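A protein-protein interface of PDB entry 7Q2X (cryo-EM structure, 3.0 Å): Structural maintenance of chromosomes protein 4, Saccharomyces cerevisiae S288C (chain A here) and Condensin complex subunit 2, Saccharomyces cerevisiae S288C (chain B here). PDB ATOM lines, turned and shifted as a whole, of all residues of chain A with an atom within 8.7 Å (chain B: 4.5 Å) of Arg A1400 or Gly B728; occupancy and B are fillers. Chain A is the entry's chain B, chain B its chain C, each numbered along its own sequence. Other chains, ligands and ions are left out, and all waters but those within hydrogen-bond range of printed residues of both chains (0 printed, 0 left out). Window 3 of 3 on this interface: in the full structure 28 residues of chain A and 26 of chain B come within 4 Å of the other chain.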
ATOM      1  N   SER A 166     -12.473   8.567 -19.795  1.00  0.00           N
ATOM      2  CA  SER A 166     -13.928   8.543 -19.679  1.00  0.00           C
ATOM      3  C   SER A 166     -14.611   8.529 -21.040  1.00  0.00           C
ATOM      4  O   SER A 166     -15.681   7.927 -21.186  1.00  0.00           O
ATOM      5  CB  SER A 166     -14.407   9.740 -18.859  1.00  0.00           C
ATOM      6  OG  SER A 166     -14.053  10.960 -19.484  1.00  0.00           O
ATOM      7  N   ALA A 168     -15.709   7.482 -24.652  1.00  0.00           N
ATOM      8  CA  ALA A 168     -15.857   6.213 -25.348  1.00  0.00           C
ATOM      9  C   ALA A 168     -16.232   6.471 -26.799  1.00  0.00           C
ATOM     10  O   ALA A 168     -17.031   7.365 -27.093  1.00  0.00           O
ATOM     11  CB  ALA A 168     -16.917   5.332 -24.681  1.00  0.00           C
ATOM     12  N   GLY A 188     -15.999  15.720 -12.019  1.00  0.00           N
ATOM     13  CA  GLY A 188     -15.912  14.342 -12.446  1.00  0.00           C
ATOM     14  C   GLY A 188     -16.354  14.078 -13.868  1.00  0.00           C
ATOM     15  O   GLY A 188     -16.248  12.933 -14.325  1.00  0.00           O
ATOM     16  N   SER A 189     -16.837  15.096 -14.584  1.00  0.00           N
ATOM     17  CA  SER A 189     -17.308  14.887 -15.950  1.00  0.00           C
ATOM     18  C   SER A 189     -16.173  14.455 -16.871  1.00  0.00           C
ATOM     19  O   SER A 189     -16.359  13.580 -17.724  1.00  0.00           O
ATOM     20  CB  SER A 189     -17.971  16.157 -16.477  1.00  0.00           C
ATOM     21  OG  SER A 189     -19.171  16.430 -15.776  1.00  0.00           O
ATOM     22  N   HIS A 219     -10.447   3.038 -22.014  1.00  0.00           N
ATOM     23  CA  HIS A 219     -11.785   3.245 -21.473  1.00  0.00           C
ATOM     24  C   HIS A 219     -12.381   1.929 -20.990  1.00  0.00           C
ATOM     25  O   HIS A 219     -12.327   0.913 -21.689  1.00  0.00           O
ATOM     26  CB  HIS A 219     -12.690   3.875 -22.530  1.00  0.00           C
ATOM     27  CG  HIS A 219     -14.117   4.006 -22.099  1.00  0.00           C
ATOM     28  ND1 HIS A 219     -14.552   5.002 -21.253  1.00  0.00           N
ATOM     29  CD2 HIS A 219     -15.209   3.260 -22.394  1.00  0.00           C
ATOM     30  CE1 HIS A 219     -15.850   4.867 -21.048  1.00  0.00           C
ATOM     31  NE2 HIS A 219     -16.273   3.819 -21.729  1.00  0.00           N
ATOM     32  N   SER A 221     -15.965   0.435 -18.955  1.00  0.00           N
ATOM     33  CA  SER A 221     -17.315   0.726 -18.492  1.00  0.00           C
ATOM     34  C   SER A 221     -18.150  -0.542 -18.599  1.00  0.00           C
ATOM     35  O   SER A 221     -17.699  -1.568 -19.113  1.00  0.00           O
ATOM     36  CB  SER A 221     -17.947   1.870 -19.288  1.00  0.00           C
ATOM     37  OG  SER A 221     -17.337   3.110 -18.975  1.00  0.00           O
ATOM     38  N   GLU A 222     -19.383  -0.456 -18.092  1.00  0.00           N
ATOM     39  CA  GLU A 222     -20.287  -1.601 -18.141  1.00  0.00           C
ATOM     40  C   GLU A 222     -20.620  -1.983 -19.578  1.00  0.00           C
ATOM     41  O   GLU A 222     -20.638  -3.170 -19.925  1.00  0.00           O
ATOM     42  CB  GLU A 222     -21.564  -1.295 -17.359  1.00  0.00           C
ATOM     43  CG  GLU A 222     -21.338  -1.002 -15.885  1.00  0.00           C
ATOM     44  CD  GLU A 222     -21.093   0.470 -15.613  1.00  0.00           C
ATOM     45  OE1 GLU A 222     -21.186   1.275 -16.564  1.00  0.00           O
ATOM     46  OE2 GLU A 222     -20.806   0.822 -14.450  1.00  0.00           O
ATOM     47  N   ALA A 223     -20.885  -0.991 -20.430  1.00  0.00           N
ATOM     48  CA  ALA A 223     -21.211  -1.262 -21.824  1.00  0.00           C
ATOM     49  C   ALA A 223     -19.987  -1.615 -22.656  1.00  0.00           C
ATOM     50  O   ALA A 223     -20.139  -2.127 -23.771  1.00  0.00           O
ATOM     51  CB  ALA A 223     -21.924  -0.058 -22.443  1.00  0.00           C
ATOM     52  N   PHE A 224     -18.782  -1.354 -22.144  1.00  0.00           N
ATOM     53  CA  PHE A 224     -17.530  -1.632 -22.843  1.00  0.00           C
ATOM     54  C   PHE A 224     -16.627  -2.420 -21.901  1.00  0.00           C
ATOM     55  O   PHE A 224     -15.720  -1.853 -21.273  1.00  0.00           O
ATOM     56  CB  PHE A 224     -16.863  -0.340 -23.309  1.00  0.00           C
ATOM     57  CG  PHE A 224     -17.634   0.391 -24.372  1.00  0.00           C
ATOM     58  CD1 PHE A 224     -17.569  -0.012 -25.695  1.00  0.00           C
ATOM     59  CD2 PHE A 224     -18.428   1.478 -24.046  1.00  0.00           C
ATOM     60  CE1 PHE A 224     -18.279   0.657 -26.674  1.00  0.00           C
ATOM     61  CE2 PHE A 224     -19.139   2.152 -25.021  1.00  0.00           C
ATOM     62  CZ  PHE A 224     -19.065   1.740 -26.336  1.00  0.00           C
ATOM     63  N   VAL A1397     -18.259  19.447 -20.981  1.00  0.00           N
ATOM     64  CA  VAL A1397     -18.261  17.990 -21.002  1.00  0.00           C
ATOM     65  C   VAL A1397     -19.330  17.485 -20.042  1.00  0.00           C
ATOM     66  O   VAL A1397     -19.478  18.004 -18.929  1.00  0.00           O
ATOM     67  CB  VAL A1397     -16.876  17.410 -20.638  1.00  0.00           C
ATOM     68  CG1 VAL A1397     -15.888  17.656 -21.767  1.00  0.00           C
ATOM     69  CG2 VAL A1397     -16.364  18.016 -19.343  1.00  0.00           C
ATOM     70  N   TYR A1398     -20.087  16.481 -20.481  1.00  0.00           N
ATOM     71  CA  TYR A1398     -21.125  15.871 -19.662  1.00  0.00           C
ATOM     72  C   TYR A1398     -21.007  14.355 -19.727  1.00  0.00           C
ATOM     73  O   TYR A1398     -20.719  13.792 -20.787  1.00  0.00           O
ATOM     74  CB  TYR A1398     -22.528  16.319 -20.107  1.00  0.00           C
ATOM     75  CG  TYR A1398     -22.826  16.111 -21.575  1.00  0.00           C
ATOM     76  CD1 TYR A1398     -22.538  17.099 -22.508  1.00  0.00           C
ATOM     77  CD2 TYR A1398     -23.414  14.936 -22.026  1.00  0.00           C
ATOM     78  CE1 TYR A1398     -22.815  16.917 -23.849  1.00  0.00           C
ATOM     79  CE2 TYR A1398     -23.695  14.747 -23.365  1.00  0.00           C
ATOM     80  CZ  TYR A1398     -23.393  15.740 -24.273  1.00  0.00           C
ATOM     81  OH  TYR A1398     -23.670  15.557 -25.608  1.00  0.00           O
ATOM     82  N   LYS A1399     -21.234  13.700 -18.591  1.00  0.00           N
ATOM     83  CA  LYS A1399     -21.063  12.259 -18.464  1.00  0.00           C
ATOM     84  C   LYS A1399     -22.408  11.576 -18.264  1.00  0.00           C
ATOM     85  O   LYS A1399     -23.200  11.986 -17.409  1.00  0.00           O
ATOM     86  CB  LYS A1399     -20.133  11.915 -17.299  1.00  0.00           C
ATOM     87  CG  LYS A1399     -19.447  10.563 -17.441  1.00  0.00           C
ATOM     88  CD  LYS A1399     -18.254  10.431 -16.509  1.00  0.00           C
ATOM     89  CE  LYS A1399     -18.557  11.001 -15.134  1.00  0.00           C
ATOM     90  NZ  LYS A1399     -19.481  10.130 -14.357  1.00  0.00           N
ATOM     91  N   ARG A1400     -22.661  10.541 -19.060  1.00  0.00           N
ATOM     92  CA  ARG A1400     -23.787   9.639 -18.867  1.00  0.00           C
ATOM     93  C   ARG A1400     -23.279   8.208 -18.952  1.00  0.00           C
ATOM     94  O   ARG A1400     -22.588   7.852 -19.911  1.00  0.00           O
ATOM     95  CB  ARG A1400     -24.885   9.873 -19.909  1.00  0.00           C
ATOM     96  CG  ARG A1400     -25.531  11.244 -19.841  1.00  0.00           C
ATOM     97  CD  ARG A1400     -26.680  11.357 -20.829  1.00  0.00           C
ATOM     98  NE  ARG A1400     -27.783  10.467 -20.488  1.00  0.00           N
ATOM     99  CZ  ARG A1400     -28.116   9.385 -21.178  1.00  0.00           C
ATOM    100  NH1 ARG A1400     -27.447   9.024 -22.261  1.00  0.00           N
ATOM    101  NH2 ARG A1400     -29.144   8.646 -20.772  1.00  0.00           N
ATOM    102  N   ASP A1401     -23.625   7.397 -17.949  1.00  0.00           N
ATOM    103  CA  ASP A1401     -23.212   5.993 -17.891  1.00  0.00           C
ATOM    104  C   ASP A1401     -21.699   5.854 -18.033  1.00  0.00           C
ATOM    105  O   ASP A1401     -21.198   4.992 -18.759  1.00  0.00           O
ATOM    106  CB  ASP A1401     -23.940   5.162 -18.947  1.00  0.00           C
ATOM    107  CG  ASP A1401     -25.369   4.843 -18.555  1.00  0.00           C
ATOM    108  OD1 ASP A1401     -25.679   4.888 -17.346  1.00  0.00           O
ATOM    109  OD2 ASP A1401     -26.182   4.547 -19.456  1.00  0.00           O
ATOM    110  N   ASN A1402     -20.967   6.727 -17.335  1.00  0.00           N
ATOM    111  CA  ASN A1402     -19.503   6.750 -17.360  1.00  0.00           C
ATOM    112  C   ASN A1402     -18.959   6.975 -18.769  1.00  0.00           C
ATOM    113  O   ASN A1402     -17.880   6.490 -19.114  1.00  0.00           O
ATOM    114  CB  ASN A1402     -18.913   5.472 -16.755  1.00  0.00           C
ATOM    115  CG  ASN A1402     -19.171   5.360 -15.265  1.00  0.00           C
ATOM    116  OD1 ASN A1402     -19.062   6.341 -14.530  1.00  0.00           O
ATOM    117  ND2 ASN A1402     -19.514   4.160 -14.813  1.00  0.00           N
ATOM    118  N   ARG A1403     -19.702   7.712 -19.591  1.00  0.00           N
ATOM    119  CA  ARG A1403     -19.274   8.074 -20.936  1.00  0.00           C
ATOM    120  C   ARG A1403     -19.375   9.583 -21.083  1.00  0.00           C
ATOM    121  O   ARG A1403     -20.442  10.157 -20.852  1.00  0.00           O
ATOM    122  CB  ARG A1403     -20.125   7.372 -21.997  1.00  0.00           C
ATOM    123  CG  ARG A1403     -19.669   5.962 -22.320  1.00  0.00           C
ATOM    124  CD  ARG A1403     -20.545   5.327 -23.386  1.00  0.00           C
ATOM    125  NE  ARG A1403     -21.388   4.271 -22.836  1.00  0.00           N
ATOM    126  CZ  ARG A1403     -22.705   4.357 -22.703  1.00  0.00           C
ATOM    127  NH1 ARG A1403     -23.368   5.440 -23.071  1.00  0.00           N
ATOM    128  NH2 ARG A1403     -23.372   3.328 -22.188  1.00  0.00           N
ATOM    129  N   THR A1404     -18.275  10.221 -21.471  1.00  0.00           N
ATOM    130  CA  THR A1404     -18.186  11.674 -21.503  1.00  0.00           C
ATOM    131  C   THR A1404     -18.293  12.181 -22.936  1.00  0.00           C
ATOM    132  O   THR A1404     -17.607  11.679 -23.832  1.00  0.00           O
ATOM    133  CB  THR A1404     -16.877  12.153 -20.872  1.00  0.00           C
ATOM    134  OG1 THR A1404     -16.846  11.774 -19.490  1.00  0.00           O
ATOM    135  CG2 THR A1404     -16.761  13.664 -20.971  1.00  0.00           C
ATOM    136  N   LYS A1405     -19.152  13.176 -23.142  1.00  0.00           N
ATOM    137  CA  LYS A1405     -19.335  13.823 -24.434  1.00  0.00           C
ATOM    138  C   LYS A1405     -19.085  15.319 -24.290  1.00  0.00           C
ATOM    139  O   LYS A1405     -19.449  15.924 -23.276  1.00  0.00           O
ATOM    140  CB  LYS A1405     -20.741  13.574 -24.985  1.00  0.00           C
ATOM    141  CG  LYS A1405     -21.024  12.121 -25.329  1.00  0.00           C
ATOM    142  CD  LYS A1405     -21.973  12.007 -26.508  1.00  0.00           C
ATOM    143  CE  LYS A1405     -22.833  10.759 -26.403  1.00  0.00           C
ATOM    144  NZ  LYS A1405     -22.073   9.611 -25.839  1.00  0.00           N
ATOM    145  N   ALA B 724     -27.877  17.272 -18.371  1.00  0.00           N
ATOM    146  CA  ALA B 724     -27.419  16.141 -19.170  1.00  0.00           C
ATOM    147  C   ALA B 724     -26.698  15.115 -18.304  1.00  0.00           C
ATOM    148  O   ALA B 724     -26.765  13.910 -18.568  1.00  0.00           O
ATOM    149  CB  ALA B 724     -26.512  16.627 -20.300  1.00  0.00           C
ATOM    150  N   GLU B 726     -27.401  14.418 -15.104  1.00  0.00           N
ATOM    151  CA  GLU B 726     -28.388  13.637 -14.362  1.00  0.00           C
ATOM    152  C   GLU B 726     -29.390  12.963 -15.297  1.00  0.00           C
ATOM    153  O   GLU B 726     -29.524  11.734 -15.298  1.00  0.00           O
ATOM    154  CB  GLU B 726     -29.109  14.514 -13.335  1.00  0.00           C
ATOM    155  CG  GLU B 726     -28.228  15.545 -12.658  1.00  0.00           C
ATOM    156  CD  GLU B 726     -29.028  16.541 -11.847  1.00  0.00           C
ATOM    157  OE1 GLU B 726     -30.271  16.550 -11.979  1.00  0.00           O
ATOM    158  OE2 GLU B 726     -28.419  17.313 -11.078  1.00  0.00           O
ATOM    159  N   HIS B 727     -30.096  13.748 -16.102  1.00  0.00           N
ATOM    160  CA  HIS B 727     -31.144  13.233 -16.970  1.00  0.00           C
ATOM    161  C   HIS B 727     -30.572  12.811 -18.318  1.00  0.00           C
ATOM    162  O   HIS B 727     -29.455  13.171 -18.695  1.00  0.00           O
ATOM    163  CB  HIS B 727     -32.245  14.281 -17.161  1.00  0.00           C
ATOM    164  CG  HIS B 727     -32.867  14.742 -15.881  1.00  0.00           C
ATOM    165  ND1 HIS B 727     -33.504  15.958 -15.758  1.00  0.00           N
ATOM    166  CD2 HIS B 727     -32.955  14.147 -14.668  1.00  0.00           C
ATOM    167  CE1 HIS B 727     -33.953  16.095 -14.523  1.00  0.00           C
ATOM    168  NE2 HIS B 727     -33.634  15.009 -13.841  1.00  0.00           N
ATOM    169  N   GLY B 728     -31.365  12.034 -19.052  1.00  0.00           N
ATOM    170  CA  GLY B 728     -30.951  11.540 -20.350  1.00  0.00           C
ATOM    171  C   GLY B 728     -31.139  12.559 -21.452  1.00  0.00           C
ATOM    172  O   GLY B 728     -32.059  12.442 -22.268  1.00  0.00           O
ATOM    173  N   LEU B 729     -30.271  13.566 -21.486  1.00  0.00           N
ATOM    174  CA  LEU B 729     -30.357  14.653 -22.447  1.00  0.00           C
ATOM    175  C   LEU B 729     -29.061  14.731 -23.242  1.00  0.00           C
ATOM    176  O   LEU B 729     -27.971  14.571 -22.684  1.00  0.00           O
ATOM    177  CB  LEU B 729     -30.622  15.985 -21.739  1.00  0.00           C
ATOM    178  CG  LEU B 729     -31.128  17.132 -22.610  1.00  0.00           C
ATOM    179  CD1 LEU B 729     -32.510  16.792 -23.146  1.00  0.00           C
ATOM    180  CD2 LEU B 729     -31.152  18.436 -21.830  1.00  0.00           C
ATOM    181  N   GLN B 730     -29.183  14.973 -24.545  1.00  0.00           N
ATOM    182  CA  GLN B 730     -28.039  15.073 -25.439  1.00  0.00           C
ATOM    183  C   GLN B 730     -27.923  16.495 -25.971  1.00  0.00           C
ATOM    184  O   GLN B 730     -28.932  17.135 -26.280  1.00  0.00           O
ATOM    185  CB  GLN B 730     -28.162  14.088 -26.607  1.00  0.00           C
ATOM    186  CG  GLN B 730     -27.623  12.698 -26.312  1.00  0.00           C
ATOM    187  CD  GLN B 730     -28.694  11.754 -25.797  1.00  0.00           C
ATOM    188  OE1 GLN B 730     -29.652  12.177 -25.149  1.00  0.00           O
ATOM    189  NE2 GLN B 730     -28.538  10.468 -26.088  1.00  0.00           N
ATOM    190  N   GLU B 745     -34.439  12.269 -26.870  1.00  0.00           N
ATOM    191  CA  GLU B 745     -34.881  10.882 -26.920  1.00  0.00           C
ATOM    192  C   GLU B 745     -34.250  10.080 -25.787  1.00  0.00           C
ATOM    193  O   GLU B 745     -33.190  10.430 -25.261  1.00  0.00           O
ATOM    194  CB  GLU B 745     -34.555  10.234 -28.268  1.00  0.00           C
ATOM    195  CG  GLU B 745     -34.714  11.138 -29.472  1.00  0.00           C
ATOM    196  CD  GLU B 745     -34.220  10.493 -30.752  1.00  0.00           C
ATOM    197  OE1 GLU B 745     -33.244   9.716 -30.690  1.00  0.00           O
ATOM    198  OE2 GLU B 745     -34.807  10.763 -31.822  1.00  0.00           O
ATOM    199  N   ASP B 746     -34.926   8.992 -25.412  1.00  0.00           N
ATOM    200  CA  ASP B 746     -34.521   8.146 -24.287  1.00  0.00           C
ATOM    201  C   ASP B 746     -34.383   8.970 -23.006  1.00  0.00           C
ATOM    202  O   ASP B 746     -33.415   8.840 -22.253  1.00  0.00           O
ATOM    203  CB  ASP B 746     -33.229   7.390 -24.603  1.00  0.00           C
ATOM    204  CG  ASP B 746     -33.002   6.209 -23.678  1.00  0.00           C
ATOM    205  OD1 ASP B 746     -33.849   5.968 -22.792  1.00  0.00           O
ATOM    206  OD2 ASP B 746     -31.974   5.519 -23.840  1.00  0.00           O
ATOM    207  N   LEU B 747     -35.368   9.828 -22.763  1.00  0.00           N
ATOM    208  CA  LEU B 747     -35.378  10.669 -21.571  1.00  0.00           C
ATOM    209  C   LEU B 747     -36.220  10.043 -20.465  1.00  0.00           C
ATOM    210  O   LEU B 747     -37.361   9.642 -20.691  1.00  0.00           O
ATOM    211  CB  LEU B 747     -35.902  12.066 -21.905  1.00  0.00           C
ATOM    212  CG  LEU B 747     -35.941  13.073 -20.755  1.00  0.00           C
ATOM    213  CD1 LEU B 747     -34.540  13.327 -20.218  1.00  0.00           C
ATOM    214  CD2 LEU B 747     -36.592  14.371 -21.206  1.00  0.00           C
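The backbone NH of Lys A1405 lies within hydrogen-bond range of the backbone carbonyl oxygen of Tyr A1398, 2.9 Å away.
Among the printed residues, pairs that only touch across the chains: Arg A1400 with Ala B724 (3.2 Å), Arg A1400 with Gly B728 (3.3 Å), Arg A1400 with His B727 (3.6 Å), Tyr A1398 with Ala B724 (3.9 Å) and Arg A1400 with Leu B729 (3.9 Å).
Printed residues of chain B that touch a printed residue of chain A: Ala B724, His B727, Gly B728 and Leu B729.
Of the 18 printed residues of chain A, 2 touch a printed residue of chain B.
Hydrophobic or aromatic side chains of chain A within 4 Å of the printed part of chain B: Tyr A1398.
Arg A1400 touches just these residues of chain B: Ala B724, His B727, Gly B728 and Leu B729.
Thr A1404 touches none of the printed residues of chain B.
Of the printed residues of chain A, Ala B724 touches Tyr A1398 (3.9 Å) and Arg A1400 (3.2 Å).
Gly B728 touches just one residue of chain A: Arg A1400 (3.3 Å).
Printed residues of chain A within 4 Å of Leu B729: Arg A1400 (3.9 Å).
Asp B746 touches none of the printed residues of chain A.
The nearest residue of chain A that does not touch Gly B728 is Tyr A1398 (8.0 Å).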
